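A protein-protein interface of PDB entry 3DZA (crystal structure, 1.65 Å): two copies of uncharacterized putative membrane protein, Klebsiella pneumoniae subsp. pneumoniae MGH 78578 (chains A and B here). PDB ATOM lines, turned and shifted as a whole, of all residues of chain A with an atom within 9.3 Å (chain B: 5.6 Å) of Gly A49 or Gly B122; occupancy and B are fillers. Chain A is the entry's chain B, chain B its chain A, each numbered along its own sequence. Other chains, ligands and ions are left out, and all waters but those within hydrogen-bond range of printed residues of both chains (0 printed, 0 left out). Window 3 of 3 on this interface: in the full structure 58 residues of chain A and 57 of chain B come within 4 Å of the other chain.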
ATOM      1  N   ALA A  42      24.259  13.452  13.486  1.00  0.00           N
ATOM      2  CA  ALA A  42      22.999  14.219  13.647  1.00  0.00           C
ATOM      3  C   ALA A  42      21.815  13.294  13.392  1.00  0.00           C
ATOM      4  O   ALA A  42      20.807  13.329  14.120  1.00  0.00           O
ATOM      5  CB  ALA A  42      22.936  15.433  12.675  1.00  0.00           C
ATOM      6  N   ARG A  43      21.914  12.471  12.356  1.00  0.00           N
ATOM      7  CA  ARG A  43      20.816  11.526  12.063  1.00  0.00           C
ATOM      8  C   ARG A  43      20.669  10.545  13.252  1.00  0.00           C
ATOM      9  O   ARG A  43      19.557  10.207  13.698  1.00  0.00           O
ATOM     10  CB  ARG A  43      21.057  10.806  10.731  1.00  0.00           C
ATOM     11  CG  ARG A  43      21.007  11.712   9.501  1.00  0.00           C
ATOM     12  CD  ARG A  43      21.256  10.910   8.229  1.00  0.00           C
ATOM     13  NE  ARG A  43      20.148   9.995   8.066  1.00  0.00           N
ATOM     14  CZ  ARG A  43      20.214   8.743   7.597  1.00  0.00           C
ATOM     15  NH1 ARG A  43      21.367   8.235   7.177  1.00  0.00           N
ATOM     16  NH2 ARG A  43      19.108   8.002   7.532  1.00  0.00           N
ATOM     17  N   LEU A  44      21.793  10.088  13.762  1.00  0.00           N
ATOM     18  CA  LEU A  44      21.784   9.166  14.907  1.00  0.00           C
ATOM     19  C   LEU A  44      21.084   9.834  16.097  1.00  0.00           C
ATOM     20  O   LEU A  44      20.182   9.249  16.716  1.00  0.00           O
ATOM     21  CB  LEU A  44      23.210   8.726  15.244  1.00  0.00           C
ATOM     22  CG  LEU A  44      23.462   7.499  16.096  1.00  0.00           C
ATOM     23  CD1 LEU A  44      22.935   6.239  15.368  1.00  0.00           C
ATOM     24  CD2 LEU A  44      24.975   7.426  16.426  1.00  0.00           C
ATOM     25  N   ALA A  45      21.448  11.080  16.371  1.00  0.00           N
ATOM     26  CA  ALA A  45      20.902  11.850  17.500  1.00  0.00           C
ATOM     27  C   ALA A  45      19.384  12.004  17.399  1.00  0.00           C
ATOM     28  O   ALA A  45      18.672  11.820  18.391  1.00  0.00           O
ATOM     29  CB  ALA A  45      21.581  13.217  17.583  1.00  0.00           C
ATOM     30  N   LEU A  46      18.888  12.301  16.196  1.00  0.00           N
ATOM     31  CA  LEU A  46      17.448  12.457  15.954  1.00  0.00           C
ATOM     32  C   LEU A  46      16.719  11.209  16.406  1.00  0.00           C
ATOM     33  O   LEU A  46      15.747  11.290  17.186  1.00  0.00           O
ATOM     34  CB  LEU A  46      17.171  12.717  14.484  1.00  0.00           C
ATOM     35  CG  LEU A  46      17.569  14.093  13.971  1.00  0.00           C
ATOM     36  CD1 LEU A  46      17.330  14.173  12.472  1.00  0.00           C
ATOM     37  CD2 LEU A  46      16.860  15.225  14.759  1.00  0.00           C
ATOM     38  N   PHE A  47      17.223  10.043  15.999  1.00  0.00           N
ATOM     39  CA  PHE A  47      16.551   8.799  16.352  1.00  0.00           C
ATOM     40  C   PHE A  47      16.799   8.287  17.766  1.00  0.00           C
ATOM     41  O   PHE A  47      16.318   7.230  18.100  1.00  0.00           O
ATOM     42  CB  PHE A  47      16.828   7.736  15.328  1.00  0.00           C
ATOM     43  CG  PHE A  47      16.146   8.004  14.011  1.00  0.00           C
ATOM     44  CD1 PHE A  47      14.747   7.969  13.925  1.00  0.00           C
ATOM     45  CD2 PHE A  47      16.872   8.355  12.879  1.00  0.00           C
ATOM     46  CE1 PHE A  47      14.104   8.219  12.716  1.00  0.00           C
ATOM     47  CE2 PHE A  47      16.229   8.612  11.685  1.00  0.00           C
ATOM     48  CZ  PHE A  47      14.842   8.547  11.599  1.00  0.00           C
ATOM     49  N   HIS A  48      17.582   9.023  18.566  1.00  0.00           N
ATOM     50  CA  HIS A  48      17.683   8.757  19.994  1.00  0.00           C
ATOM     51  C   HIS A  48      16.848   9.775  20.809  1.00  0.00           C
ATOM     52  O   HIS A  48      17.004   9.846  22.048  1.00  0.00           O
ATOM     53  CB  HIS A  48      19.148   8.782  20.446  1.00  0.00           C
ATOM     54  CG  HIS A  48      19.938   7.587  20.018  1.00  0.00           C
ATOM     55  ND1 HIS A  48      20.324   7.377  18.706  1.00  0.00           N
ATOM     56  CD2 HIS A  48      20.424   6.536  20.728  1.00  0.00           C
ATOM     57  CE1 HIS A  48      21.031   6.260  18.639  1.00  0.00           C
ATOM     58  NE2 HIS A  48      21.120   5.741  19.854  1.00  0.00           N
ATOM     59  N   GLY A  49      15.996  10.554  20.131  1.00  0.00           N
ATOM     60  CA  GLY A  49      15.215  11.619  20.778  1.00  0.00           C
ATOM     61  C   GLY A  49      16.092  12.724  21.362  1.00  0.00           C
ATOM     62  O   GLY A  49      15.829  13.237  22.455  1.00  0.00           O
ATOM     63  N   GLN A  50      17.153  13.070  20.620  1.00  0.00           N
ATOM     64  CA  GLN A  50      18.098  14.127  20.989  1.00  0.00           C
ATOM     65  C   GLN A  50      18.155  15.245  19.948  1.00  0.00           C
ATOM     66  O   GLN A  50      19.195  15.482  19.311  1.00  0.00           O
ATOM     67  CB  GLN A  50      19.483  13.518  21.218  1.00  0.00           C
ATOM     68  CG  GLN A  50      19.474  12.460  22.310  1.00  0.00           C
ATOM     69  CD  GLN A  50      20.745  11.643  22.320  1.00  0.00           C
ATOM     70  OE1 GLN A  50      21.573  11.756  21.410  1.00  0.00           O
ATOM     71  NE2 GLN A  50      20.873  10.760  23.301  1.00  0.00           N
ATOM     72  N   PRO A  51      17.031  15.955  19.761  1.00  0.00           N
ATOM     73  CA  PRO A  51      17.013  17.032  18.757  1.00  0.00           C
ATOM     74  C   PRO A  51      17.972  18.198  19.020  1.00  0.00           C
ATOM     75  O   PRO A  51      18.428  18.828  18.067  1.00  0.00           O
ATOM     76  CB  PRO A  51      15.550  17.490  18.763  1.00  0.00           C
ATOM     77  CG  PRO A  51      15.056  17.132  20.119  1.00  0.00           C
ATOM     78  CD  PRO A  51      15.714  15.806  20.418  1.00  0.00           C
ATOM     79  N   ASP A  52      18.290  18.480  20.288  1.00  0.00           N
ATOM     80  CA  ASP A  52      19.206  19.585  20.619  1.00  0.00           C
ATOM     81  C   ASP A  52      20.602  19.227  20.120  1.00  0.00           C
ATOM     82  O   ASP A  52      21.297  20.065  19.507  1.00  0.00           O
ATOM     83  CB  ASP A  52      19.241  19.891  22.136  1.00  0.00           C
ATOM     84  CG  ASP A  52      17.926  20.416  22.676  1.00  0.00           C
ATOM     85  OD1 ASP A  52      17.071  20.853  21.887  1.00  0.00           O
ATOM     86  OD2 ASP A  52      17.783  20.383  23.922  1.00  0.00           O
ATOM     87  N   SER A  53      20.997  17.979  20.357  1.00  0.00           N
ATOM     88  CA  SER A  53      22.264  17.452  19.830  1.00  0.00           C
ATOM     89  C   SER A  53      22.304  17.481  18.303  1.00  0.00           C
ATOM     90  O   SER A  53      23.324  17.876  17.718  1.00  0.00           O
ATOM     91  CB  SER A  53      22.505  16.052  20.370  1.00  0.00           C
ATOM     92  OG  SER A  53      23.773  15.613  19.997  1.00  0.00           O
ATOM     93  N   ALA A  54      21.222  17.051  17.655  1.00  0.00           N
ATOM     94  CA  ALA A  54      21.133  17.075  16.195  1.00  0.00           C
ATOM     95  C   ALA A  54      21.343  18.499  15.670  1.00  0.00           C
ATOM     96  O   ALA A  54      22.077  18.719  14.713  1.00  0.00           O
ATOM     97  CB  ALA A  54      19.788  16.469  15.712  1.00  0.00           C
ATOM     98  N   TYR A 166      11.670  16.460  12.191  1.00  0.00           N
ATOM     99  CA  TYR A 166      12.852  15.640  12.428  1.00  0.00           C
ATOM    100  C   TYR A 166      13.066  14.503  11.422  1.00  0.00           C
ATOM    101  O   TYR A 166      14.190  14.333  10.891  1.00  0.00           O
ATOM    102  CB  TYR A 166      12.835  15.122  13.856  1.00  0.00           C
ATOM    103  CG  TYR A 166      12.745  16.214  14.901  1.00  0.00           C
ATOM    104  CD1 TYR A 166      13.633  17.280  14.915  1.00  0.00           C
ATOM    105  CD2 TYR A 166      11.738  16.191  15.852  1.00  0.00           C
ATOM    106  CE1 TYR A 166      13.534  18.287  15.876  1.00  0.00           C
ATOM    107  CE2 TYR A 166      11.641  17.184  16.810  1.00  0.00           C
ATOM    108  CZ  TYR A 166      12.532  18.225  16.810  1.00  0.00           C
ATOM    109  OH  TYR A 166      12.401  19.203  17.777  1.00  0.00           O
ATOM    110  N   LYS B 118       6.864  12.979  19.187  1.00  0.00           N
ATOM    111  CA  LYS B 118       7.449  12.106  20.208  1.00  0.00           C
ATOM    112  C   LYS B 118       8.951  12.354  20.372  1.00  0.00           C
ATOM    113  O   LYS B 118       9.439  12.498  21.475  1.00  0.00           O
ATOM    114  CB  LYS B 118       7.176  10.640  19.864  1.00  0.00           C
ATOM    115  CG  LYS B 118       5.702  10.316  19.975  1.00  0.00           C
ATOM    116  CD  LYS B 118       5.371   8.882  19.644  1.00  0.00           C
ATOM    117  CE  LYS B 118       3.859   8.723  19.589  1.00  0.00           C
ATOM    118  NZ  LYS B 118       3.475   7.297  19.514  1.00  0.00           N
ATOM    119  N   LEU B 119       9.681  12.465  19.258  1.00  0.00           N
ATOM    120  CA  LEU B 119      11.116  12.735  19.331  1.00  0.00           C
ATOM    121  C   LEU B 119      11.383  14.099  19.973  1.00  0.00           C
ATOM    122  O   LEU B 119      12.380  14.264  20.674  1.00  0.00           O
ATOM    123  CB  LEU B 119      11.767  12.655  17.934  1.00  0.00           C
ATOM    124  CG  LEU B 119      11.798  11.287  17.251  1.00  0.00           C
ATOM    125  CD1 LEU B 119      12.247  11.410  15.753  1.00  0.00           C
ATOM    126  CD2 LEU B 119      12.667  10.267  18.038  1.00  0.00           C
ATOM    127  N   ALA B 120      10.510  15.073  19.710  1.00  0.00           N
ATOM    128  CA  ALA B 120      10.639  16.398  20.329  1.00  0.00           C
ATOM    129  C   ALA B 120      10.664  16.304  21.846  1.00  0.00           C
ATOM    130  O   ALA B 120      11.339  17.093  22.509  1.00  0.00           O
ATOM    131  CB  ALA B 120       9.499  17.330  19.882  1.00  0.00           C
ATOM    132  N   LYS B 121       9.932  15.326  22.383  1.00  0.00           N
ATOM    133  CA  LYS B 121       9.801  15.103  23.820  1.00  0.00           C
ATOM    134  C   LYS B 121      10.755  14.016  24.348  1.00  0.00           C
ATOM    135  O   LYS B 121      10.653  13.611  25.501  1.00  0.00           O
ATOM    136  CB  LYS B 121       8.353  14.688  24.110  1.00  0.00           C
ATOM    137  CG  LYS B 121       7.364  15.808  23.931  1.00  0.00           C
ATOM    138  CD  LYS B 121       5.948  15.386  24.303  1.00  0.00           C
ATOM    139  CE  LYS B 121       5.039  16.599  24.517  1.00  0.00           C
ATOM    140  NZ  LYS B 121       3.605  16.239  24.406  1.00  0.00           N
ATOM    141  N   GLY B 122      11.656  13.520  23.501  1.00  0.00           N
ATOM    142  CA  GLY B 122      12.599  12.468  23.891  1.00  0.00           C
ATOM    143  C   GLY B 122      12.009  11.071  24.013  1.00  0.00           C
ATOM    144  O   GLY B 122      12.632  10.173  24.597  1.00  0.00           O
ATOM    145  N   ASP B 123      10.807  10.884  23.470  1.00  0.00           N
ATOM    146  CA  ASP B 123      10.118   9.594  23.491  1.00  0.00           C
ATOM    147  C   ASP B 123      10.591   8.765  22.301  1.00  0.00           C
ATOM    148  O   ASP B 123       9.867   8.560  21.339  1.00  0.00           O
ATOM    149  CB  ASP B 123       8.595   9.794  23.496  1.00  0.00           C
ATOM    150  CG  ASP B 123       7.807   8.471  23.445  1.00  0.00           C
ATOM    151  OD1 ASP B 123       8.393   7.412  23.683  1.00  0.00           O
ATOM    152  OD2 ASP B 123       6.590   8.506  23.151  1.00  0.00           O
ATOM    153  N   GLN B 124      11.822   8.279  22.398  1.00  0.00           N
ATOM    154  CA  GLN B 124      12.423   7.478  21.307  1.00  0.00           C
ATOM    155  C   GLN B 124      11.624   6.205  20.995  1.00  0.00           C
ATOM    156  O   GLN B 124      11.331   5.906  19.825  1.00  0.00           O
ATOM    157  CB  GLN B 124      13.855   7.110  21.682  1.00  0.00           C
ATOM    158  CG  GLN B 124      14.546   6.208  20.686  1.00  0.00           C
ATOM    159  CD  GLN B 124      15.758   5.500  21.252  1.00  0.00           C
ATOM    160  OE1 GLN B 124      15.758   5.071  22.398  1.00  0.00           O
ATOM    161  NE2 GLN B 124      16.798   5.346  20.429  1.00  0.00           N
ATOM    162  N   LYS B 125      11.325   5.415  22.028  1.00  0.00           N
ATOM    163  CA  LYS B 125      10.576   4.181  21.826  1.00  0.00           C
ATOM    164  C   LYS B 125       9.245   4.436  21.107  1.00  0.00           C
ATOM    165  O   LYS B 125       8.906   3.729  20.163  1.00  0.00           O
ATOM    166  CB  LYS B 125      10.313   3.425  23.132  1.00  0.00           C
ATOM    167  CG  LYS B 125       9.542   2.144  22.846  1.00  0.00           C
ATOM    168  CD  LYS B 125       9.308   1.251  24.042  1.00  0.00           C
ATOM    169  CE  LYS B 125       8.179   0.233  23.728  1.00  0.00           C
ATOM    170  NZ  LYS B 125       8.439  -0.689  22.567  1.00  0.00           N
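No position is printed for both chains.
Of the 7 pairs that touch across the chains among the printed residues, none has its exchanged pair printed and touching as well.
Printed residues of chain B that touch a printed residue of chain A: Leu B119, Ala B120, Gly B122 and Gln B124.
Hydrophobic or aromatic side chains of chain B within 4 Å of the printed part of chain A: Leu B119 and Ala B120.
Among the printed residues, 7 pairs touch across the chains.
Among the printed residues, no Asp or Glu carboxylate lies within 4 Å of a Lys or Arg side-chain nitrogen of the other chain.
Gly B122 touches just one residue of chain A: Gly A49 (3.6 Å).
Of the printed residues of chain B, Tyr A166 touches Ala B120 (3.7 Å).
Printed residues of chain B within 4 Å of His A48: Gln B124.
Printed residues of chain B within 4 Å of Pro A51: Leu B119.
Of the printed residues of chain A, Gln B124 touches Phe A47 and His A48.
Of the printed residues of chain A, Leu B119 touches Leu A46 (3.4 Å), Gly A49 (3.9 Å) and Pro A51 (3.7 Å).
The nearest residue of chain B that does not touch Gly A49 is Gln B124 (4.3 Å).
The nearest printed residue of chain B that does not touch His A48 is Leu B119 (5.0 Å).
CD2 of Leu B119 touches O of Leu A46, 3.4 Å away.
Gln B124 touches His A48 (NE2 to CA, 3.6 Å).
Leu B119 touches Gly A49 (O to CA, 3.9 Å).
O of Gly A49 touches CA of Gly B122 (3.6 Å).
O of Leu B119 touches CD of Pro A51, 3.7 Å away.
Tyr A166 touches Ala B120.
A ring nitrogen (ND1) of His A48 is in hydrogen-bond range of the backbone carbonyl oxygen (O) of Leu A44, at 2.7 Å.
NE2 of Gln B124 sits at hydrogen-bond distance from O of Phe A47 (3.0 Å).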
